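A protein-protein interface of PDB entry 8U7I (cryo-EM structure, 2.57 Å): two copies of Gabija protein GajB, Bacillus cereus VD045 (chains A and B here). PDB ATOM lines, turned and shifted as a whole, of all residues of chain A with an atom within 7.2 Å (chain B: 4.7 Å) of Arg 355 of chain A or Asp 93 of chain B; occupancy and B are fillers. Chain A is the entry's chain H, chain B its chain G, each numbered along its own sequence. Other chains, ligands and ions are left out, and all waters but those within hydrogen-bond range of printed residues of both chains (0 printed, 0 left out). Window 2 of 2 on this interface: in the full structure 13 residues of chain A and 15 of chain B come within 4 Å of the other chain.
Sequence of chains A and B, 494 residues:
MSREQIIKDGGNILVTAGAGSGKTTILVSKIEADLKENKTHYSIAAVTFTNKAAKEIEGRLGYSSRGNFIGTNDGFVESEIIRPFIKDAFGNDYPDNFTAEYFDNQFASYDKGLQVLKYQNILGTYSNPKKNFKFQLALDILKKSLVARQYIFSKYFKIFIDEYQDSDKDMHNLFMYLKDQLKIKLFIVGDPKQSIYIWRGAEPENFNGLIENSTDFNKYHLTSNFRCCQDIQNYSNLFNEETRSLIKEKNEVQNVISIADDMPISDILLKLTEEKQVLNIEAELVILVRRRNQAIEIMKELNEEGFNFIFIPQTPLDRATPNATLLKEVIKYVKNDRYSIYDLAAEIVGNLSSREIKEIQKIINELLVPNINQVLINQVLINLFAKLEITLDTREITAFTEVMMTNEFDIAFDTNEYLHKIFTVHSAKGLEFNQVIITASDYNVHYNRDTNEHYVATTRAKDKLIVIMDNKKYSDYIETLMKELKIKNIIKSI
Of the printed residues of chain B, Glu 101 of chain A touches Tyr 119. Of chain B, only Asp 93 (3.6 Å), Lys 118 (3.6 Å) and Tyr 119 (3.2 Å) come within 4 Å of Arg 355 of chain A. Asp 93 of chain B touches just these residues of chain A: Ser 354 (3.5 Å), Arg 355 (3.6 Å) and Lys 358 (3.9 Å). Printed residues of chain A within 4 Å of Tyr 119 of chain B: Glu 101 (3.4 Å) and Arg 355 (3.2 Å). The nearest printed residue of chain B that does not touch Ser 354 of chain A is Tyr 94 of chain B (5.3 Å).
Hydrophobic or aromatic side chains of chain B that line the printed part of chain A: Tyr 119. Among the printed residues, 8 pairs touch across the chains.
Among the printed residues, pairs that only touch across the chains: Arg 355 of chain A with Tyr 119 of chain B (3.2 Å), Ser 354 of chain A with Asp 93 of chain B (3.5 Å), Arg 355 of chain A with Asp 93 of chain B (3.6 Å), Arg 355 of chain A with Lys 118 of chain B (3.6 Å), Lys 358 of chain A with Asn 92 of chain B (3.7 Å) and Lys 358 of chain A with Asp 93 of chain B (3.9 Å).
No position is printed for both chains. Of the 8 pairs that touch across the chains among the printed residues, none has its exchanged pair printed and touching as well.
The side-chain amino group (NZ) of Lys 118 of chain B lies within salt-bridge range of the side-chain carboxylate (OD2) of Asp 93 of chain B, 3.1 Å away. NH1 of Arg 355 of chain A is in salt-bridge range of OE1 of Glu 101 of chain A (2.9 Å). OD1 of Asp 104 of chain A lies within salt-bridge range of NH2 of Arg 355 of chain A (2.4 Å). OG of Ser 353 of chain A sits close to N of Arg 355 of chain A, 3.3 Å away.
The backbone carbonyl oxygen of Asn 92 of chain B sits at hydrogen-bond distance from the side-chain hydroxyl of Ser 354 of chain A, at 2.7 Å. The side-chain carboxylate of Glu 101 of chain A lies close to the backbone carbonyl oxygen of Tyr 119 of chain B (3.4 Å).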
ATOM      1  N   GLU A 101      16.575  23.658  15.142  1.00  0.00           N
ATOM      2  CA  GLU A 101      17.782  22.869  14.913  1.00  0.00           C
ATOM      3  C   GLU A 101      18.183  23.019  13.451  1.00  0.00           C
ATOM      4  O   GLU A 101      17.480  22.537  12.558  1.00  0.00           O
ATOM      5  CB  GLU A 101      17.560  21.402  15.274  1.00  0.00           C
ATOM      6  CG  GLU A 101      17.370  21.159  16.762  1.00  0.00           C
ATOM      7  CD  GLU A 101      17.185  19.694  17.094  1.00  0.00           C
ATOM      8  OE1 GLU A 101      16.999  18.890  16.157  1.00  0.00           O
ATOM      9  OE2 GLU A 101      17.231  19.343  18.292  1.00  0.00           O
ATOM     10  N   PHE A 103      21.058  21.893  11.946  1.00  0.00           N
ATOM     11  CA  PHE A 103      21.922  20.880  11.356  1.00  0.00           C
ATOM     12  C   PHE A 103      21.173  19.651  10.861  1.00  0.00           C
ATOM     13  O   PHE A 103      21.695  18.937   9.997  1.00  0.00           O
ATOM     14  CB  PHE A 103      22.992  20.460  12.366  1.00  0.00           C
ATOM     15  CG  PHE A 103      23.900  21.582  12.784  1.00  0.00           C
ATOM     16  CD1 PHE A 103      24.048  22.705  11.987  1.00  0.00           C
ATOM     17  CD2 PHE A 103      24.601  21.516  13.975  1.00  0.00           C
ATOM     18  CE1 PHE A 103      24.878  23.739  12.369  1.00  0.00           C
ATOM     19  CE2 PHE A 103      25.433  22.548  14.362  1.00  0.00           C
ATOM     20  CZ  PHE A 103      25.573  23.660  13.558  1.00  0.00           C
ATOM     21  N   ASP A 104      19.976  19.382  11.374  1.00  0.00           N
ATOM     22  CA  ASP A 104      19.257  18.164  11.033  1.00  0.00           C
ATOM     23  C   ASP A 104      17.810  18.481  10.687  1.00  0.00           C
ATOM     24  O   ASP A 104      17.323  19.597  10.892  1.00  0.00           O
ATOM     25  CB  ASP A 104      19.321  17.143  12.176  1.00  0.00           C
ATOM     26  CG  ASP A 104      20.735  16.888  12.648  1.00  0.00           C
ATOM     27  OD1 ASP A 104      21.248  17.695  13.452  1.00  0.00           O
ATOM     28  OD2 ASP A 104      21.335  15.882  12.217  1.00  0.00           O
ATOM     29  N   ASN A 105      17.129  17.466  10.151  1.00  0.00           N
ATOM     30  CA  ASN A 105      15.714  17.550   9.790  1.00  0.00           C
ATOM     31  C   ASN A 105      15.457  18.659   8.773  1.00  0.00           C
ATOM     32  O   ASN A 105      14.465  19.384   8.855  1.00  0.00           O
ATOM     33  CB  ASN A 105      14.840  17.734  11.032  1.00  0.00           C
ATOM     34  CG  ASN A 105      15.197  16.766  12.143  1.00  0.00           C
ATOM     35  OD1 ASN A 105      16.152  16.983  12.889  1.00  0.00           O
ATOM     36  ND2 ASN A 105      14.431  15.688  12.258  1.00  0.00           N
ATOM     37  N   LEU A 352      21.369  28.915  18.596  1.00  0.00           N
ATOM     38  CA  LEU A 352      21.968  27.593  18.471  1.00  0.00           C
ATOM     39  C   LEU A 352      21.433  26.682  19.566  1.00  0.00           C
ATOM     40  O   LEU A 352      21.405  27.065  20.741  1.00  0.00           O
ATOM     41  CB  LEU A 352      23.494  27.677  18.549  1.00  0.00           C
ATOM     42  CG  LEU A 352      24.252  27.541  17.225  1.00  0.00           C
ATOM     43  CD1 LEU A 352      24.324  26.084  16.798  1.00  0.00           C
ATOM     44  CD2 LEU A 352      23.608  28.388  16.139  1.00  0.00           C
ATOM     45  N   SER A 353      21.008  25.483  19.178  1.00  0.00           N
ATOM     46  CA  SER A 353      20.516  24.510  20.142  1.00  0.00           C
ATOM     47  C   SER A 353      21.646  24.032  21.047  1.00  0.00           C
ATOM     48  O   SER A 353      22.815  23.998  20.655  1.00  0.00           O
ATOM     49  CB  SER A 353      19.882  23.319  19.423  1.00  0.00           C
ATOM     50  OG  SER A 353      19.773  22.201  20.287  1.00  0.00           O
ATOM     51  N   SER A 354      21.279  23.657  22.276  1.00  0.00           N
ATOM     52  CA  SER A 354      22.274  23.198  23.240  1.00  0.00           C
ATOM     53  C   SER A 354      22.987  21.948  22.744  1.00  0.00           C
ATOM     54  O   SER A 354      24.207  21.814  22.903  1.00  0.00           O
ATOM     55  CB  SER A 354      21.615  22.937  24.593  1.00  0.00           C
ATOM     56  OG  SER A 354      21.389  21.551  24.789  1.00  0.00           O
ATOM     57  N   ARG A 355      22.241  21.016  22.146  1.00  0.00           N
ATOM     58  CA  ARG A 355      22.867  19.830  21.572  1.00  0.00           C
ATOM     59  C   ARG A 355      23.817  20.206  20.442  1.00  0.00           C
ATOM     60  O   ARG A 355      24.916  19.648  20.332  1.00  0.00           O
ATOM     61  CB  ARG A 355      21.794  18.862  21.073  1.00  0.00           C
ATOM     62  CG  ARG A 355      22.270  17.927  19.979  1.00  0.00           C
ATOM     63  CD  ARG A 355      21.111  17.216  19.312  1.00  0.00           C
ATOM     64  NE  ARG A 355      21.400  16.922  17.914  1.00  0.00           N
ATOM     65  CZ  ARG A 355      20.537  17.088  16.922  1.00  0.00           C
ATOM     66  NH1 ARG A 355      19.309  17.524  17.140  1.00  0.00           N
ATOM     67  NH2 ARG A 355      20.914  16.798  15.681  1.00  0.00           N
ATOM     68  N   GLU A 356      23.412  21.154  19.594  1.00  0.00           N
ATOM     69  CA  GLU A 356      24.282  21.600  18.511  1.00  0.00           C
ATOM     70  C   GLU A 356      25.537  22.274  19.052  1.00  0.00           C
ATOM     71  O   GLU A 356      26.630  22.096  18.502  1.00  0.00           O
ATOM     72  CB  GLU A 356      23.516  22.542  17.581  1.00  0.00           C
ATOM     73  CG  GLU A 356      22.427  21.855  16.772  1.00  0.00           C
ATOM     74  CD  GLU A 356      21.723  22.799  15.817  1.00  0.00           C
ATOM     75  OE1 GLU A 356      21.842  24.029  15.998  1.00  0.00           O
ATOM     76  OE2 GLU A 356      21.052  22.311  14.884  1.00  0.00           O
ATOM     77  N   ILE A 357      25.399  23.056  20.125  1.00  0.00           N
ATOM     78  CA  ILE A 357      26.568  23.663  20.757  1.00  0.00           C
ATOM     79  C   ILE A 357      27.494  22.586  21.308  1.00  0.00           C
ATOM     80  O   ILE A 357      28.721  22.671  21.171  1.00  0.00           O
ATOM     81  CB  ILE A 357      26.133  24.653  21.853  1.00  0.00           C
ATOM     82  CG1 ILE A 357      25.377  25.833  21.238  1.00  0.00           C
ATOM     83  CG2 ILE A 357      27.337  25.148  22.637  1.00  0.00           C
ATOM     84  CD1 ILE A 357      24.373  26.468  22.174  1.00  0.00           C
ATOM     85  N   LYS A 358      26.923  21.556  21.939  1.00  0.00           N
ATOM     86  CA  LYS A 358      27.738  20.463  22.460  1.00  0.00           C
ATOM     87  C   LYS A 358      28.473  19.739  21.338  1.00  0.00           C
ATOM     88  O   LYS A 358      29.639  19.358  21.499  1.00  0.00           O
ATOM     89  CB  LYS A 358      26.868  19.486  23.250  1.00  0.00           C
ATOM     90  CG  LYS A 358      26.559  19.939  24.665  1.00  0.00           C
ATOM     91  CD  LYS A 358      25.975  18.806  25.492  1.00  0.00           C
ATOM     92  CE  LYS A 358      25.714  19.249  26.922  1.00  0.00           C
ATOM     93  NZ  LYS A 358      26.963  19.697  27.598  1.00  0.00           N
ATOM     94  N   GLU A 359      27.807  19.534  20.200  1.00  0.00           N
ATOM     95  CA  GLU A 359      28.484  18.949  19.047  1.00  0.00           C
ATOM     96  C   GLU A 359      29.602  19.858  18.552  1.00  0.00           C
ATOM     97  O   GLU A 359      30.677  19.380  18.167  1.00  0.00           O
ATOM     98  CB  GLU A 359      27.474  18.665  17.934  1.00  0.00           C
ATOM     99  CG  GLU A 359      28.092  18.480  16.559  1.00  0.00           C
ATOM    100  CD  GLU A 359      27.951  19.712  15.691  1.00  0.00           C
ATOM    101  OE1 GLU A 359      27.196  20.626  16.081  1.00  0.00           O
ATOM    102  OE2 GLU A 359      28.599  19.771  14.626  1.00  0.00           O
ATOM    103  N   ILE A 360      29.368  21.172  18.557  1.00  0.00           N
ATOM    104  CA  ILE A 360      30.429  22.121  18.232  1.00  0.00           C
ATOM    105  C   ILE A 360      31.568  22.011  19.238  1.00  0.00           C
ATOM    106  O   ILE A 360      32.748  22.085  18.875  1.00  0.00           O
ATOM    107  CB  ILE A 360      29.864  23.553  18.166  1.00  0.00           C
ATOM    108  CG1 ILE A 360      29.003  23.745  16.913  1.00  0.00           C
ATOM    109  CG2 ILE A 360      30.984  24.582  18.195  1.00  0.00           C
ATOM    110  CD1 ILE A 360      29.431  22.904  15.726  1.00  0.00           C
ATOM    111  N   GLN A 361      31.236  21.826  20.517  1.00  0.00           N
ATOM    112  CA  GLN A 361      32.276  21.697  21.534  1.00  0.00           C
ATOM    113  C   GLN A 361      33.121  20.448  21.312  1.00  0.00           C
ATOM    114  O   GLN A 361      34.350  20.496  21.438  1.00  0.00           O
ATOM    115  CB  GLN A 361      31.649  21.676  22.927  1.00  0.00           C
ATOM    116  CG  GLN A 361      32.649  21.880  24.053  1.00  0.00           C
ATOM    117  CD  GLN A 361      31.993  21.912  25.418  1.00  0.00           C
ATOM    118  OE1 GLN A 361      30.787  21.698  25.544  1.00  0.00           O
ATOM    119  NE2 GLN A 361      32.784  22.182  26.449  1.00  0.00           N
ATOM    120  N   LYS A 362      32.485  19.322  20.976  1.00  0.00           N
ATOM    121  CA  LYS A 362      33.229  18.075  20.831  1.00  0.00           C
ATOM    122  C   LYS A 362      34.071  18.058  19.562  1.00  0.00           C
ATOM    123  O   LYS A 362      35.022  17.274  19.464  1.00  0.00           O
ATOM    124  CB  LYS A 362      32.271  16.882  20.858  1.00  0.00           C
ATOM    125  CG  LYS A 362      31.896  16.335  19.490  1.00  0.00           C
ATOM    126  CD  LYS A 362      30.988  15.123  19.617  1.00  0.00           C
ATOM    127  CE  LYS A 362      29.541  15.531  19.840  1.00  0.00           C
ATOM    128  NZ  LYS A 362      28.778  15.590  18.565  1.00  0.00           N
ATOM    129  N   LYS A 387      29.448  21.030   8.412  1.00  0.00           N
ATOM    130  CA  LYS A 387      28.315  21.133   9.324  1.00  0.00           C
ATOM    131  C   LYS A 387      27.593  22.464   9.155  1.00  0.00           C
ATOM    132  O   LYS A 387      26.358  22.518   9.180  1.00  0.00           O
ATOM    133  CB  LYS A 387      28.782  20.953  10.768  1.00  0.00           C
ATOM    134  CG  LYS A 387      28.605  19.541  11.301  1.00  0.00           C
ATOM    135  CD  LYS A 387      27.140  19.136  11.315  1.00  0.00           C
ATOM    136  CE  LYS A 387      26.840  18.175  12.453  1.00  0.00           C
ATOM    137  NZ  LYS A 387      25.485  17.574  12.333  1.00  0.00           N
ATOM    138  N   PHE B  90      21.224  12.758  31.326  1.00  0.00           N
ATOM    139  CA  PHE B  90      21.729  12.525  29.978  1.00  0.00           C
ATOM    140  C   PHE B  90      22.365  13.763  29.355  1.00  0.00           C
ATOM    141  O   PHE B  90      22.556  13.806  28.137  1.00  0.00           O
ATOM    142  CB  PHE B  90      20.607  12.006  29.078  1.00  0.00           C
ATOM    143  CG  PHE B  90      20.206  10.591  29.365  1.00  0.00           C
ATOM    144  CD1 PHE B  90      21.163   9.611  29.547  1.00  0.00           C
ATOM    145  CD2 PHE B  90      18.873  10.242  29.454  1.00  0.00           C
ATOM    146  CE1 PHE B  90      20.795   8.309  29.810  1.00  0.00           C
ATOM    147  CE2 PHE B  90      18.501   8.942  29.718  1.00  0.00           C
ATOM    148  CZ  PHE B  90      19.463   7.975  29.896  1.00  0.00           C
ATOM    149  N   GLY B  91      22.700  14.768  30.153  1.00  0.00           N
ATOM    150  CA  GLY B  91      23.320  15.968  29.636  1.00  0.00           C
ATOM    151  C   GLY B  91      22.307  16.970  29.115  1.00  0.00           C
ATOM    152  O   GLY B  91      21.126  16.680  28.917  1.00  0.00           O
ATOM    153  N   ASN B  92      22.798  18.188  28.877  1.00  0.00           N
ATOM    154  CA  ASN B  92      21.924  19.282  28.468  1.00  0.00           C
ATOM    155  C   ASN B  92      21.412  19.129  27.043  1.00  0.00           C
ATOM    156  O   ASN B  92      20.484  19.844  26.655  1.00  0.00           O
ATOM    157  CB  ASN B  92      22.656  20.615  28.609  1.00  0.00           C
ATOM    158  CG  ASN B  92      22.702  21.102  30.039  1.00  0.00           C
ATOM    159  OD1 ASN B  92      21.682  21.145  30.724  1.00  0.00           O
ATOM    160  ND2 ASN B  92      23.891  21.471  30.500  1.00  0.00           N
ATOM    161  N   ASP B  93      21.998  18.225  26.256  1.00  0.00           N
ATOM    162  CA  ASP B  93      21.559  18.055  24.874  1.00  0.00           C
ATOM    163  C   ASP B  93      20.119  17.563  24.804  1.00  0.00           C
ATOM    164  O   ASP B  93      19.332  18.040  23.978  1.00  0.00           O
ATOM    165  CB  ASP B  93      22.490  17.089  24.146  1.00  0.00           C
ATOM    166  CG  ASP B  93      22.872  15.899  24.996  1.00  0.00           C
ATOM    167  OD1 ASP B  93      22.766  15.997  26.236  1.00  0.00           O
ATOM    168  OD2 ASP B  93      23.278  14.866  24.426  1.00  0.00           O
ATOM    169  N   TYR B  94      19.758  16.613  25.659  1.00  0.00           N
ATOM    170  CA  TYR B  94      18.416  16.053  25.624  1.00  0.00           C
ATOM    171  C   TYR B  94      17.393  17.105  26.045  1.00  0.00           C
ATOM    172  O   TYR B  94      17.683  17.951  26.896  1.00  0.00           O
ATOM    173  CB  TYR B  94      18.316  14.836  26.539  1.00  0.00           C
ATOM    174  CG  TYR B  94      19.006  13.607  26.002  1.00  0.00           C
ATOM    175  CD1 TYR B  94      20.387  13.553  25.899  1.00  0.00           C
ATOM    176  CD2 TYR B  94      18.276  12.499  25.600  1.00  0.00           C
ATOM    177  CE1 TYR B  94      21.023  12.430  25.411  1.00  0.00           C
ATOM    178  CE2 TYR B  94      18.903  11.372  25.112  1.00  0.00           C
ATOM    179  CZ  TYR B  94      20.276  11.343  25.019  1.00  0.00           C
ATOM    180  OH  TYR B  94      20.905  10.222  24.532  1.00  0.00           O
ATOM    181  N   PRO B  95      16.196  17.083  25.469  1.00  0.00           N
ATOM    182  CA  PRO B  95      15.193  18.099  25.783  1.00  0.00           C
ATOM    183  C   PRO B  95      14.251  17.669  26.899  1.00  0.00           C
ATOM    184  O   PRO B  95      14.098  16.487  27.211  1.00  0.00           O
ATOM    185  CB  PRO B  95      14.432  18.241  24.459  1.00  0.00           C
ATOM    186  CG  PRO B  95      14.559  16.881  23.807  1.00  0.00           C
ATOM    187  CD  PRO B  95      15.722  16.148  24.437  1.00  0.00           C
ATOM    188  N   LYS B 118      17.104  12.091  21.265  1.00  0.00           N
ATOM    189  CA  LYS B 118      17.786  13.373  21.394  1.00  0.00           C
ATOM    190  C   LYS B 118      17.459  14.296  20.225  1.00  0.00           C
ATOM    191  O   LYS B 118      17.140  15.474  20.421  1.00  0.00           O
ATOM    192  CB  LYS B 118      19.295  13.152  21.503  1.00  0.00           C
ATOM    193  CG  LYS B 118      20.108  14.433  21.576  1.00  0.00           C
ATOM    194  CD  LYS B 118      21.566  14.183  21.231  1.00  0.00           C
ATOM    195  CE  LYS B 118      22.103  12.955  21.946  1.00  0.00           C
ATOM    196  NZ  LYS B 118      23.589  12.970  22.030  1.00  0.00           N
ATOM    197  N   TYR B 119      17.525  13.773  19.000  1.00  0.00           N
ATOM    198  CA  TYR B 119      17.295  14.603  17.823  1.00  0.00           C
ATOM    199  C   TYR B 119      15.818  14.887  17.583  1.00  0.00           C
ATOM    200  O   TYR B 119      15.469  15.996  17.164  1.00  0.00           O
ATOM    201  CB  TYR B 119      17.906  13.943  16.586  1.00  0.00           C
ATOM    202  CG  TYR B 119      19.228  13.256  16.843  1.00  0.00           C
ATOM    203  CD1 TYR B 119      20.260  13.916  17.494  1.00  0.00           C
ATOM    204  CD2 TYR B 119      19.445  11.951  16.429  1.00  0.00           C
ATOM    205  CE1 TYR B 119      21.470  13.297  17.729  1.00  0.00           C
ATOM    206  CE2 TYR B 119      20.654  11.324  16.659  1.00  0.00           C
ATOM    207  CZ  TYR B 119      21.661  12.001  17.310  1.00  0.00           C
ATOM    208  OH  TYR B 119      22.866  11.378  17.542  1.00  0.00           O
